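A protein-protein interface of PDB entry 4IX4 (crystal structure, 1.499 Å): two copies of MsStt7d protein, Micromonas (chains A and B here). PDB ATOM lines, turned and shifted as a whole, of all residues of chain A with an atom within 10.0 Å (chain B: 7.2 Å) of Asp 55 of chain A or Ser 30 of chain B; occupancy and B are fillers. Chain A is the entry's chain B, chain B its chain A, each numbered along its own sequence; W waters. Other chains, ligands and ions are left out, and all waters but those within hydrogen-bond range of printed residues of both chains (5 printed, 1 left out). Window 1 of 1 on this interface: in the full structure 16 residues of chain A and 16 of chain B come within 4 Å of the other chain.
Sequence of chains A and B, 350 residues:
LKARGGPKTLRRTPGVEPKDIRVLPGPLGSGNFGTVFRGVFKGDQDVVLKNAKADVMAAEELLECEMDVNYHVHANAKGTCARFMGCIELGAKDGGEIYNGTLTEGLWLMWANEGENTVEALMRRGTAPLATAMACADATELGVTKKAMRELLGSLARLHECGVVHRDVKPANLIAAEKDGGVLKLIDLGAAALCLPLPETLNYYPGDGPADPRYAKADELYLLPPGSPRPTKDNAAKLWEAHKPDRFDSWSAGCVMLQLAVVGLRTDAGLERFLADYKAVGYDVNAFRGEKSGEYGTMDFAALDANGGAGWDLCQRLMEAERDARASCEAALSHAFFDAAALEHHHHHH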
ATOM      1  N   PRO A  27       4.507 -17.030 -20.178  1.00  0.00           N
ATOM      2  CA  PRO A  27       4.490 -16.006 -21.227  1.00  0.00           C
ATOM      3  C   PRO A  27       5.895 -15.709 -21.736  1.00  0.00           C
ATOM      4  O   PRO A  27       6.862 -15.770 -20.968  1.00  0.00           O
ATOM      5  CB  PRO A  27       3.923 -14.785 -20.505  1.00  0.00           C
ATOM      6  CG  PRO A  27       3.073 -15.355 -19.428  1.00  0.00           C
ATOM      7  CD  PRO A  27       3.783 -16.596 -18.970  1.00  0.00           C
ATOM      8  N   GLY A  29       6.833 -12.805 -23.053  1.00  0.00           N
ATOM      9  CA  GLY A  29       7.183 -11.408 -22.838  1.00  0.00           C
ATOM     10  C   GLY A  29       6.078 -10.595 -22.190  1.00  0.00           C
ATOM     11  O   GLY A  29       4.914 -10.986 -22.222  1.00  0.00           O
ATOM     12  N   SER A  30       6.445  -9.457 -21.605  1.00  0.00           N
ATOM     13  CA  SER A  30       5.475  -8.571 -20.970  1.00  0.00           C
ATOM     14  C   SER A  30       4.254  -8.378 -21.863  1.00  0.00           C
ATOM     15  O   SER A  30       3.118  -8.551 -21.422  1.00  0.00           O
ATOM     16  CB  SER A  30       6.117  -7.218 -20.654  1.00  0.00           C
ATOM     17  OG  SER A  30       5.183  -6.328 -20.072  1.00  0.00           O
ATOM     18  N   GLY A  31       4.496  -8.023 -23.121  1.00  0.00           N
ATOM     19  CA  GLY A  31       3.424  -7.898 -24.088  1.00  0.00           C
ATOM     20  C   GLY A  31       2.693  -6.574 -24.020  1.00  0.00           C
ATOM     21  O   GLY A  31       2.627  -5.929 -22.973  1.00  0.00           O
ATOM     22  N   ASN A  32       2.127  -6.166 -25.153  1.00  0.00           N
ATOM     23  CA  ASN A  32       1.349  -4.936 -25.223  1.00  0.00           C
ATOM     24  C   ASN A  32      -0.091  -5.164 -24.777  1.00  0.00           C
ATOM     25  O   ASN A  32      -0.399  -5.102 -23.587  1.00  0.00           O
ATOM     26  CB  ASN A  32       1.380  -4.362 -26.640  1.00  0.00           C
ATOM     27  CG  ASN A  32       0.918  -2.919 -26.694  1.00  0.00           C
ATOM     28  OD1 ASN A  32      -0.196  -2.595 -26.281  1.00  0.00           O
ATOM     29  ND2 ASN A  32       1.774  -2.042 -27.207  1.00  0.00           N
ATOM     30  N   PHE A  33      -0.969  -5.432 -25.739  1.00  0.00           N
ATOM     31  CA  PHE A  33      -2.368  -5.723 -25.437  1.00  0.00           C
ATOM     32  C   PHE A  33      -2.625  -7.223 -25.418  1.00  0.00           C
ATOM     33  O   PHE A  33      -3.772  -7.652 -25.331  1.00  0.00           O
ATOM     34  CB  PHE A  33      -3.280  -5.093 -26.494  1.00  0.00           C
ATOM     35  CG  PHE A  33      -2.913  -5.477 -27.906  1.00  0.00           C
ATOM     36  CD1 PHE A  33      -3.344  -6.676 -28.450  1.00  0.00           C
ATOM     37  CD2 PHE A  33      -2.120  -4.638 -28.686  1.00  0.00           C
ATOM     38  CE1 PHE A  33      -2.986  -7.040 -29.751  1.00  0.00           C
ATOM     39  CE2 PHE A  33      -1.760  -4.988 -29.987  1.00  0.00           C
ATOM     40  CZ  PHE A  33      -2.204  -6.196 -30.523  1.00  0.00           C
ATOM     41  N   GLY A  34      -1.564  -8.017 -25.534  1.00  0.00           N
ATOM     42  CA  GLY A  34      -1.708  -9.460 -25.606  1.00  0.00           C
ATOM     43  C   GLY A  34      -0.568 -10.208 -24.941  1.00  0.00           C
ATOM     44  O   GLY A  34       0.430  -9.603 -24.531  1.00  0.00           O
ATOM     45  N   THR A  35      -0.719 -11.526 -24.837  1.00  0.00           N
ATOM     46  CA  THR A  35       0.267 -12.383 -24.195  1.00  0.00           C
ATOM     47  C   THR A  35       0.644 -13.506 -25.139  1.00  0.00           C
ATOM     48  O   THR A  35      -0.217 -14.087 -25.787  1.00  0.00           O
ATOM     49  CB  THR A  35      -0.298 -13.005 -22.909  1.00  0.00           C
ATOM     50  OG1 THR A  35      -0.846 -11.971 -22.083  1.00  0.00           O
ATOM     51  CG2 THR A  35       0.786 -13.755 -22.155  1.00  0.00           C
ATOM     52  N   VAL A  36       1.941 -13.782 -25.228  1.00  0.00           N
ATOM     53  CA  VAL A  36       2.472 -14.763 -26.161  1.00  0.00           C
ATOM     54  C   VAL A  36       3.004 -15.988 -25.408  1.00  0.00           C
ATOM     55  O   VAL A  36       3.686 -15.853 -24.388  1.00  0.00           O
ATOM     56  CB  VAL A  36       3.592 -14.124 -27.017  1.00  0.00           C
ATOM     57  CG1 VAL A  36       4.287 -15.162 -27.859  1.00  0.00           C
ATOM     58  CG2 VAL A  36       3.019 -13.022 -27.895  1.00  0.00           C
ATOM     59  N   ASN A  51      -2.913 -14.410 -27.291  1.00  0.00           N
ATOM     60  CA  ASN A  51      -4.284 -14.002 -27.006  1.00  0.00           C
ATOM     61  C   ASN A  51      -4.307 -12.566 -26.482  1.00  0.00           C
ATOM     62  O   ASN A  51      -3.249 -11.967 -26.297  1.00  0.00           O
ATOM     63  CB  ASN A  51      -4.976 -14.989 -26.048  1.00  0.00           C
ATOM     64  CG  ASN A  51      -4.480 -14.882 -24.616  1.00  0.00           C
ATOM     65  OD1 ASN A  51      -3.401 -14.352 -24.354  1.00  0.00           O
ATOM     66  ND2 ASN A  51      -5.269 -15.410 -23.680  1.00  0.00           N
ATOM     67  N   ALA A  52      -5.499 -12.006 -26.272  1.00  0.00           N
ATOM     68  CA  ALA A  52      -5.612 -10.645 -25.751  1.00  0.00           C
ATOM     69  C   ALA A  52      -5.468 -10.630 -24.234  1.00  0.00           C
ATOM     70  O   ALA A  52      -5.808 -11.603 -23.562  1.00  0.00           O
ATOM     71  CB  ALA A  52      -6.945 -10.030 -26.145  1.00  0.00           C
ATOM     72  N   LYS A  53      -4.966  -9.520 -23.700  1.00  0.00           N
ATOM     73  CA  LYS A  53      -5.019  -9.283 -22.254  1.00  0.00           C
ATOM     74  C   LYS A  53      -6.432  -8.891 -21.840  1.00  0.00           C
ATOM     75  O   LYS A  53      -7.033  -7.989 -22.425  1.00  0.00           O
ATOM     76  CB  LYS A  53      -4.035  -8.189 -21.843  1.00  0.00           C
ATOM     77  CG  LYS A  53      -2.584  -8.628 -21.924  1.00  0.00           C
ATOM     78  CD  LYS A  53      -1.653  -7.462 -21.665  1.00  0.00           C
ATOM     79  CE  LYS A  53      -0.197  -7.868 -21.743  1.00  0.00           C
ATOM     80  NZ  LYS A  53       0.703  -6.735 -21.368  1.00  0.00           N
ATOM     81  N   ALA A  54      -6.960  -9.578 -20.830  1.00  0.00           N
ATOM     82  CA  ALA A  54      -8.323  -9.325 -20.365  1.00  0.00           C
ATOM     83  C   ALA A  54      -8.483  -7.948 -19.720  1.00  0.00           C
ATOM     84  O   ALA A  54      -9.599  -7.430 -19.615  1.00  0.00           O
ATOM     85  CB  ALA A  54      -8.759 -10.406 -19.396  1.00  0.00           C
ATOM     86  N   ASP A  55      -7.375  -7.362 -19.281  1.00  0.00           N
ATOM     87  CA  ASP A  55      -7.430  -6.129 -18.507  1.00  0.00           C
ATOM     88  C   ASP A  55      -7.186  -4.868 -19.327  1.00  0.00           C
ATOM     89  O   ASP A  55      -7.160  -3.766 -18.787  1.00  0.00           O
ATOM     90  CB  ASP A  55      -6.467  -6.202 -17.313  1.00  0.00           C
ATOM     91  CG  ASP A  55      -5.016  -6.400 -17.728  1.00  0.00           C
ATOM     92  OD1 ASP A  55      -4.755  -7.050 -18.754  1.00  0.00           O
ATOM     93  OD2 ASP A  55      -4.126  -5.913 -17.006  1.00  0.00           O
ATOM     94  N   VAL A  56      -7.010  -5.038 -20.634  1.00  0.00           N
ATOM     95  CA  VAL A  56      -6.699  -3.916 -21.508  1.00  0.00           C
ATOM     96  C   VAL A  56      -7.878  -3.525 -22.388  1.00  0.00           C
ATOM     97  O   VAL A  56      -8.444  -4.357 -23.105  1.00  0.00           O
ATOM     98  CB  VAL A  56      -5.471  -4.233 -22.380  1.00  0.00           C
ATOM     99  CG1 VAL A  56      -5.256  -3.134 -23.419  1.00  0.00           C
ATOM    100  CG2 VAL A  56      -4.256  -4.412 -21.487  1.00  0.00           C
ATOM    101  N   MET A  57      -8.248  -2.252 -22.324  1.00  0.00           N
ATOM    102  CA  MET A  57      -9.371  -1.735 -23.102  1.00  0.00           C
ATOM    103  C   MET A  57      -9.203  -2.022 -24.595  1.00  0.00           C
ATOM    104  O   MET A  57      -8.148  -1.757 -25.172  1.00  0.00           O
ATOM    105  CB  MET A  57      -9.527  -0.231 -22.866  1.00  0.00           C
ATOM    106  CG  MET A  57     -10.714   0.394 -23.579  1.00  0.00           C
ATOM    107  SD  MET A  57     -12.290  -0.313 -23.076  1.00  0.00           S
ATOM    108  CE  MET A  57     -12.228   0.003 -21.319  1.00  0.00           C
ATOM    109  N   ALA A  58     -10.240  -2.578 -25.215  1.00  0.00           N
ATOM    110  CA  ALA A  58     -10.218  -2.872 -26.657  1.00  0.00           C
ATOM    111  C   ALA A  58      -9.069  -3.772 -27.136  1.00  0.00           C
ATOM    112  O   ALA A  58      -8.714  -3.744 -28.316  1.00  0.00           O
ATOM    113  CB  ALA A  58     -10.231  -1.571 -27.459  1.00  0.00           C
ATOM    114  N   ALA A  59      -8.493  -4.566 -26.237  1.00  0.00           N
ATOM    115  CA  ALA A  59      -7.452  -5.513 -26.627  1.00  0.00           C
ATOM    116  C   ALA A  59      -7.961  -6.469 -27.688  1.00  0.00           C
ATOM    117  O   ALA A  59      -7.212  -6.865 -28.571  1.00  0.00           O
ATOM    118  CB  ALA A  59      -6.936  -6.287 -25.421  1.00  0.00           C
ATOM    119  N   GLU A  60      -9.229  -6.856 -27.607  1.00  0.00           N
ATOM    120  CA  GLU A  60      -9.737  -7.787 -28.601  1.00  0.00           C
ATOM    121  C   GLU A  60      -9.756  -7.100 -29.966  1.00  0.00           C
ATOM    122  O   GLU A  60      -9.418  -7.711 -30.970  1.00  0.00           O
ATOM    123  CB  GLU A  60     -11.099  -8.379 -28.216  1.00  0.00           C
ATOM    124  CG  GLU A  60     -12.285  -7.564 -28.597  1.00  0.00           C
ATOM    125  CD  GLU A  60     -13.545  -8.116 -27.980  1.00  0.00           C
ATOM    126  OE1 GLU A  60     -14.040  -9.157 -28.470  1.00  0.00           O
ATOM    127  OE2 GLU A  60     -14.022  -7.525 -26.987  1.00  0.00           O
ATOM    128  N   LEU A  62      -7.676  -4.765 -30.909  1.00  0.00           N
ATOM    129  CA  LEU A  62      -6.287  -4.668 -31.345  1.00  0.00           C
ATOM    130  C   LEU A  62      -5.779  -6.005 -31.872  1.00  0.00           C
ATOM    131  O   LEU A  62      -5.065  -6.054 -32.871  1.00  0.00           O
ATOM    132  CB  LEU A  62      -5.400  -4.157 -30.217  1.00  0.00           C
ATOM    133  CG  LEU A  62      -5.652  -2.697 -29.847  1.00  0.00           C
ATOM    134  CD1 LEU A  62      -5.087  -2.394 -28.464  1.00  0.00           C
ATOM    135  CD2 LEU A  62      -5.056  -1.773 -30.910  1.00  0.00           C
ATOM    136  N   PRO B  27       8.370 -12.143 -13.422  1.00  0.00           N
ATOM    137  CA  PRO B  27       7.411 -11.037 -13.319  1.00  0.00           C
ATOM    138  C   PRO B  27       6.037 -11.499 -12.843  1.00  0.00           C
ATOM    139  O   PRO B  27       5.620 -12.617 -13.156  1.00  0.00           O
ATOM    140  CB  PRO B  27       7.333 -10.504 -14.755  1.00  0.00           C
ATOM    141  CG  PRO B  27       7.842 -11.610 -15.616  1.00  0.00           C
ATOM    142  CD  PRO B  27       8.856 -12.336 -14.799  1.00  0.00           C
ATOM    143  N   LEU B  28       5.344 -10.636 -12.106  1.00  0.00           N
ATOM    144  CA  LEU B  28       4.085 -10.999 -11.466  1.00  0.00           C
ATOM    145  C   LEU B  28       2.863 -10.393 -12.141  1.00  0.00           C
ATOM    146  O   LEU B  28       1.742 -10.866 -11.942  1.00  0.00           O
ATOM    147  CB  LEU B  28       4.082 -10.542 -10.007  1.00  0.00           C
ATOM    148  CG  LEU B  28       5.236 -10.931  -9.089  1.00  0.00           C
ATOM    149  CD1 LEU B  28       4.967 -10.398  -7.692  1.00  0.00           C
ATOM    150  CD2 LEU B  28       5.416 -12.437  -9.062  1.00  0.00           C
ATOM    151  N   GLY B  29       3.067  -9.334 -12.912  1.00  0.00           N
ATOM    152  CA  GLY B  29       1.947  -8.571 -13.436  1.00  0.00           C
ATOM    153  C   GLY B  29       1.489  -8.944 -14.830  1.00  0.00           C
ATOM    154  O   GLY B  29       2.006  -9.884 -15.443  1.00  0.00           O
ATOM    155  N   SER B  30       0.502  -8.207 -15.332  1.00  0.00           N
ATOM    156  CA  SER B  30       0.125  -8.317 -16.737  1.00  0.00           C
ATOM    157  C   SER B  30       1.094  -7.492 -17.586  1.00  0.00           C
ATOM    158  O   SER B  30       1.137  -7.638 -18.803  1.00  0.00           O
ATOM    159  CB  SER B  30      -1.332  -7.893 -16.970  1.00  0.00           C
ATOM    160  OG  SER B  30      -1.567  -6.549 -16.583  1.00  0.00           O
ATOM    161  N   GLY B  31       1.875  -6.643 -16.922  1.00  0.00           N
ATOM    162  CA  GLY B  31       2.957  -5.909 -17.555  1.00  0.00           C
ATOM    163  C   GLY B  31       2.572  -4.879 -18.602  1.00  0.00           C
ATOM    164  O   GLY B  31       3.033  -4.944 -19.739  1.00  0.00           O
ATOM    165  N   ASN B  32       1.723  -3.937 -18.200  1.00  0.00           N
ATOM    166  CA  ASN B  32       1.255  -2.879 -19.086  1.00  0.00           C
ATOM    167  C   ASN B  32       2.254  -1.731 -19.186  1.00  0.00           C
ATOM    168  O   ASN B  32       2.895  -1.550 -20.221  1.00  0.00           O
ATOM    169  CB  ASN B  32      -0.104  -2.353 -18.622  1.00  0.00           C
ATOM    170  CG  ASN B  32      -1.257  -3.201 -19.121  1.00  0.00           C
ATOM    171  OD1 ASN B  32      -1.159  -3.852 -20.161  1.00  0.00           O
ATOM    172  ND2 ASN B  32      -2.359  -3.196 -18.379  1.00  0.00           N
ATOM    173  N   PHE B  33       2.385  -0.956 -18.113  1.00  0.00           N
ATOM    174  CA  PHE B  33       3.329   0.180 -18.122  1.00  0.00           C
ATOM    175  C   PHE B  33       4.539  -0.025 -17.210  1.00  0.00           C
ATOM    176  O   PHE B  33       5.514   0.722 -17.270  1.00  0.00           O
ATOM    177  CB  PHE B  33       2.648   1.562 -17.939  1.00  0.00           C
ATOM    178  CG  PHE B  33       2.581   2.080 -16.501  1.00  0.00           C
ATOM    179  CD1 PHE B  33       3.727   2.454 -15.797  1.00  0.00           C
ATOM    180  CD2 PHE B  33       1.348   2.276 -15.892  1.00  0.00           C
ATOM    181  CE1 PHE B  33       3.641   2.953 -14.491  1.00  0.00           C
ATOM    182  CE2 PHE B  33       1.251   2.774 -14.595  1.00  0.00           C
ATOM    183  CZ  PHE B  33       2.400   3.115 -13.886  1.00  0.00           C
ATOM    184  N   GLY B  34       4.485  -1.071 -16.398  1.00  0.00           N
ATOM    185  CA  GLY B  34       5.588  -1.389 -15.516  1.00  0.00           C
ATOM    186  C   GLY B  34       5.751  -2.882 -15.351  1.00  0.00           C
ATOM    187  O   GLY B  34       4.925  -3.665 -15.808  1.00  0.00           O
ATOM    188  N   VAL B  36       6.647  -5.916 -12.400  1.00  0.00           N
ATOM    189  CA  VAL B  36       6.625  -6.158 -10.965  1.00  0.00           C
ATOM    190  C   VAL B  36       7.375  -7.438 -10.615  1.00  0.00           C
ATOM    191  O   VAL B  36       7.176  -8.474 -11.260  1.00  0.00           O
ATOM    192  CB  VAL B  36       5.172  -6.241 -10.460  1.00  0.00           C
ATOM    193  CG1 VAL B  36       5.137  -6.553  -8.979  1.00  0.00           C
ATOM    194  CG2 VAL B  36       4.450  -4.936 -10.755  1.00  0.00           C
ATOM    195  N   LYS B  53       8.347   0.249 -17.743  1.00  0.00           N
ATOM    196  CA  LYS B  53       8.726  -0.452 -18.968  1.00  0.00           C
ATOM    197  C   LYS B  53       9.472   0.465 -19.933  1.00  0.00           C
ATOM    198  O   LYS B  53       9.004   1.556 -20.265  1.00  0.00           O
ATOM    199  CB  LYS B  53       7.496  -1.044 -19.653  1.00  0.00           C
ATOM    200  CG  LYS B  53       6.886  -2.225 -18.923  1.00  0.00           C
ATOM    201  CD  LYS B  53       5.624  -2.705 -19.622  1.00  0.00           C
ATOM    202  CE  LYS B  53       5.918  -3.169 -21.040  1.00  0.00           C
ATOM    203  NZ  LYS B  53       4.695  -3.735 -21.698  1.00  0.00           N
ATOM    204  N   ASP B 168      -9.144   1.375 -10.710  1.00  0.00           N
ATOM    205  CA  ASP B 168      -8.822   0.029 -11.158  1.00  0.00           C
ATOM    206  C   ASP B 168      -9.213  -1.001 -10.122  1.00  0.00           C
ATOM    207  O   ASP B 168      -8.482  -1.958  -9.870  1.00  0.00           O
ATOM    208  CB  ASP B 168      -7.343  -0.103 -11.509  1.00  0.00           C
ATOM    209  CG  ASP B 168      -7.077  -1.254 -12.461  1.00  0.00           C
ATOM    210  OD1 ASP B 168      -5.894  -1.588 -12.680  1.00  0.00           O
ATOM    211  OD2 ASP B 168      -8.055  -1.827 -12.987  1.00  0.00           O
ATOM    212  N   LYS B 170     -10.885  -4.161  -8.770  1.00  0.00           N
ATOM    213  CA  LYS B 170     -11.262  -5.473  -9.312  1.00  0.00           C
ATOM    214  C   LYS B 170     -10.624  -6.551  -8.446  1.00  0.00           C
ATOM    215  O   LYS B 170      -9.698  -6.275  -7.699  1.00  0.00           O
ATOM    216  CB  LYS B 170     -10.805  -5.630 -10.769  1.00  0.00           C
ATOM    217  CG  LYS B 170      -9.317  -5.428 -10.991  1.00  0.00           C
ATOM    218  CD  LYS B 170      -9.006  -5.376 -12.480  1.00  0.00           C
ATOM    219  CE  LYS B 170      -7.527  -5.133 -12.698  1.00  0.00           C
ATOM    220  NZ  LYS B 170      -7.236  -4.459 -13.990  1.00  0.00           N
ATOM    221  N   ALA B 172      -8.503  -8.805  -9.094  1.00  0.00           N
ATOM    222  CA  ALA B 172      -7.063  -8.932  -9.330  1.00  0.00           C
ATOM    223  C   ALA B 172      -6.222  -7.888  -8.594  1.00  0.00           C
ATOM    224  O   ALA B 172      -5.010  -8.063  -8.447  1.00  0.00           O
ATOM    225  CB  ALA B 172      -6.766  -8.880 -10.820  1.00  0.00           C
ATOM    226  N   ASP B 188      -2.041  -1.525  -6.724  1.00  0.00           N
ATOM    227  CA  ASP B 188      -2.057  -0.928  -8.054  1.00  0.00           C
ATOM    228  C   ASP B 188      -2.771   0.417  -8.115  1.00  0.00           C
ATOM    229  O   ASP B 188      -3.911   0.507  -8.572  1.00  0.00           O
ATOM    230  CB  ASP B 188      -2.681  -1.895  -9.064  1.00  0.00           C
ATOM    231  CG  ASP B 188      -2.278  -1.587 -10.492  1.00  0.00           C
ATOM    232  OD1 ASP B 188      -1.595  -0.564 -10.712  1.00  0.00           O
ATOM    233  OD2 ASP B 188      -2.643  -2.368 -11.396  1.00  0.00           O
ATOM    234  N   ALA B 211      -8.803   2.218 -18.237  1.00  0.00           N
ATOM    235  CA  ALA B 211      -9.892   1.426 -17.676  1.00  0.00           C
ATOM    236  C   ALA B 211      -9.758  -0.051 -18.020  1.00  0.00           C
ATOM    237  O   ALA B 211      -9.337  -0.405 -19.116  1.00  0.00           O
ATOM    238  CB  ALA B 211     -11.238   1.953 -18.153  1.00  0.00           C
ATOM    239  N   ASP B 212     -10.146  -0.911 -17.086  1.00  0.00           N
ATOM    240  CA  ASP B 212     -10.280  -2.333 -17.367  1.00  0.00           C
ATOM    241  C   ASP B 212     -11.683  -2.541 -17.929  1.00  0.00           C
ATOM    242  O   ASP B 212     -12.671  -2.209 -17.273  1.00  0.00           O
ATOM    243  CB  ASP B 212     -10.079  -3.130 -16.076  1.00  0.00           C
ATOM    244  CG  ASP B 212     -10.085  -4.638 -16.302  1.00  0.00           C
ATOM    245  OD1 ASP B 212     -10.975  -5.140 -17.022  1.00  0.00           O
ATOM    246  OD2 ASP B 212      -9.214  -5.329 -15.737  1.00  0.00           O
ATOM    247  N   PRO B 213     -11.783  -3.073 -19.158  1.00  0.00           N
ATOM    248  CA  PRO B 213     -13.102  -3.111 -19.801  1.00  0.00           C
ATOM    249  C   PRO B 213     -14.101  -4.003 -19.069  1.00  0.00           C
ATOM    250  O   PRO B 213     -15.306  -3.860 -19.270  1.00  0.00           O
ATOM    251  CB  PRO B 213     -12.799  -3.690 -21.188  1.00  0.00           C
ATOM    252  CG  PRO B 213     -11.518  -4.438 -21.014  1.00  0.00           C
ATOM    253  CD  PRO B 213     -10.728  -3.636 -20.014  1.00  0.00           C
ATOM    254  N   ARG B 214     -13.614  -4.902 -18.221  1.00  0.00           N
ATOM    255  CA  ARG B 214     -14.510  -5.782 -17.482  1.00  0.00           C
ATOM    256  C   ARG B 214     -15.141  -5.080 -16.276  1.00  0.00           C
ATOM    257  O   ARG B 214     -16.240  -5.438 -15.858  1.00  0.00           O
ATOM    258  CB  ARG B 214     -13.760  -7.015 -16.993  1.00  0.00           C
ATOM    259  CG  ARG B 214     -13.126  -7.836 -18.098  1.00  0.00           C
ATOM    260  CD  ARG B 214     -12.184  -8.851 -17.502  1.00  0.00           C
ATOM    261  NE  ARG B 214     -11.041  -8.176 -16.890  1.00  0.00           N
ATOM    262  CZ  ARG B 214     -10.125  -8.769 -16.134  1.00  0.00           C
ATOM    263  NH1 ARG B 214     -10.195 -10.072 -15.871  1.00  0.00           N
ATOM    264  NH2 ARG B 214      -9.125  -8.047 -15.639  1.00  0.00           N
ATOM    265  N   TYR B 215     -14.431  -4.102 -15.710  1.00  0.00           N
ATOM    266  CA  TYR B 215     -14.809  -3.517 -14.418  1.00  0.00           C
ATOM    267  C   TYR B 215     -15.147  -2.033 -14.451  1.00  0.00           C
ATOM    268  O   TYR B 215     -15.577  -1.474 -13.443  1.00  0.00           O
ATOM    269  CB  TYR B 215     -13.716  -3.769 -13.372  1.00  0.00           C
ATOM    270  CG  TYR B 215     -13.517  -5.237 -13.113  1.00  0.00           C
ATOM    271  CD1 TYR B 215     -14.366  -5.926 -12.251  1.00  0.00           C
ATOM    272  CD2 TYR B 215     -12.513  -5.950 -13.762  1.00  0.00           C
ATOM    273  CE1 TYR B 215     -14.221  -7.277 -12.027  1.00  0.00           C
ATOM    274  CE2 TYR B 215     -12.360  -7.315 -13.543  1.00  0.00           C
ATOM    275  CZ  TYR B 215     -13.220  -7.973 -12.672  1.00  0.00           C
ATOM    276  OH  TYR B 215     -13.069  -9.328 -12.451  1.00  0.00           O
ATOM    277  N   ASP B 268     -14.369 -14.390 -16.633  1.00  0.00           N
ATOM    278  CA  ASP B 268     -14.568 -13.156 -17.387  1.00  0.00           C
ATOM    279  C   ASP B 268     -15.853 -13.264 -18.205  1.00  0.00           C
ATOM    280  O   ASP B 268     -16.681 -12.357 -18.207  1.00  0.00           O
ATOM    281  CB  ASP B 268     -13.386 -12.874 -18.323  1.00  0.00           C
ATOM    282  CG  ASP B 268     -12.101 -12.553 -17.577  1.00  0.00           C
ATOM    283  OD1 ASP B 268     -12.173 -12.150 -16.399  1.00  0.00           O
ATOM    284  OD2 ASP B 268     -11.017 -12.685 -18.188  1.00  0.00           O
HETATM  285  O   HOH W   1      -1.339  -2.171 -22.569  1.00  0.00           O
HETATM  286  O   HOH W   2      -2.467  -7.031 -14.144  1.00  0.00           O
HETATM  287  O   HOH W   3      -6.956  -0.285 -20.681  1.00  0.00           O
HETATM  288  O   HOH W   4      -6.232  -1.149 -18.292  1.00  0.00           O
HETATM  289  O   HOH W   5      -6.832  -2.592 -16.296  1.00  0.00           O
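Water W5 lies within hydrogen-bond range of O of Asp 55 of chain A (2.8 Å) and NZ of Lys 170 of chain B (3.0 Å).
Water W3 bridges the backbone carbonyl oxygen of Ala 211 of chain B (2.9 Å) and the backbone NH of Met 57 of chain A (2.9 Å).
Water W1 bridges OD1 of Asn 32 of chain B and O of Asn 32 of chain A.
The guanidinium group of Arg 214 of chain B sits at hydrogen-bond distance from the backbone carbonyl oxygen of Ala 54 of chain A, 3.2 Å away.
The backbone carbonyl oxygen (O) of Ser 30 of chain A sits close to the backbone carbonyl oxygen (O) of Ser 30 of chain B (3.4 Å).
O of Gly 31 of chain B is in hydrogen-bond range of NZ of Lys 53 of chain A (3.4 Å).
The backbone carbonyl oxygen of Gly 31 of chain A lies within hydrogen-bond range of the side-chain amino group of Lys 53 of chain B.
The side-chain carboxylate of Asp 55 of chain A sits at hydrogen-bond distance from the side-chain hydroxyl of Ser 30 of chain B (2.7 Å).
The backbone carbonyl oxygen of Ser 30 of chain B is in hydrogen-bond range of the side-chain amino group of Lys 53 of chain A (2.8 Å).
The backbone carbonyl oxygen (O) of Gly 31 of chain B sits at hydrogen-bond distance from the side-chain hydroxyl (OG) of Ser 30 of chain A, at 2.6 Å.
The backbone carbonyl oxygen of Gly 31 of chain A sits close to the backbone carbonyl oxygen of Gly 31 of chain B, 3.4 Å away.
The side-chain amino group (NZ) of Lys 53 of chain B is in hydrogen-bond range of the side-chain hydroxyl (OG) of Ser 30 of chain A (3.1 Å).
Ser 30 of chain A touches Gly 31 of chain B, but with the chains exchanged Gly 31 of chain A does not touch Ser 30 of chain B (4.7 Å).
Asn 32 of chain A touches its own counterpart, Asn 32 of chain B.
Of the printed residues of chain B, Asn 32 of chain A touches Asn 32 (3.7 Å).
Ala 52 of chain A touches none of the printed residues of chain B.
Ser 30 of chain B touches three residues of chain A.
Gly 31 of chain B touches just these residues of chain A: Ser 30 (2.6 Å), Gly 31 (3.4 Å) and Lys 53 (3.4 Å).
Of chain A, only Ala 54 (3.7 Å) and Asp 55 (3.3 Å) come within 4 Å of Asp 212 of chain B.
The nearest residue of chain A that does not touch Ser 30 of chain B is Gly 31 of chain A (4.7 Å).
The nearest printed residue of chain B that does not touch Ser 30 of chain A is Asn 32 of chain B (4.6 Å).
The side-chain carboxylate (OD2) of Asp 168 of chain B lies within salt-bridge range of the side-chain amino group (NZ) of Lys 170 of chain B (2.9 Å).
NH1 of Arg 214 of chain B lies within salt-bridge range of OD1 of Asp 268 of chain B (2.9 Å).
Among the printed residues, merely in contact across the chains: Asp 55 of chain A with Asp 212 of chain B (3.3 Å), Val 56 of chain A with Asn 32 of chain B (3.4 Å), Ala 54 of chain A with Asp 268 of chain B (3.4 Å), Asp 55 of chain A with Asn 32 of chain B (3.5 Å), Met 57 of chain A with Pro 213 of chain B (3.6 Å), Lys 53 of chain A with Asn 32 of chain B (3.6 Å), Asp 55 of chain A with Arg 214 of chain B (3.6 Å), Met 57 of chain A with Ala 211 of chain B (3.7 Å), Val 56 of chain A with Pro 213 of chain B (3.7 Å), Ala 54 of chain A with Asp 212 of chain B (3.7 Å), Asn 32 of chain A with Asn 32 of chain B (3.7 Å), Asp 55 of chain A with Pro 213 of chain B (3.8 Å), Ala 54 of chain A with Pro 213 of chain B (3.8 Å) and Asp 55 of chain A with Lys 170 of chain B (3.8 Å).
Of the 20 printed residues of chain A, 8 touch a printed residue of chain B.
Printed residues of chain A that touch a printed residue of chain B: Ser 30, Gly 31, Asn 32, Lys 53, Ala 54, Asp 55, Val 56 and Met 57.
Hydrophobic or aromatic side chains of chain A that line the printed part of chain B: Ala 54, Val 56 and Met 57.
Hydrophobic or aromatic side chains of chain B within 4 Å of the printed part of chain A: Ala 211 and Pro 213.
Among the printed residues, 23 pairs touch across the chains.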
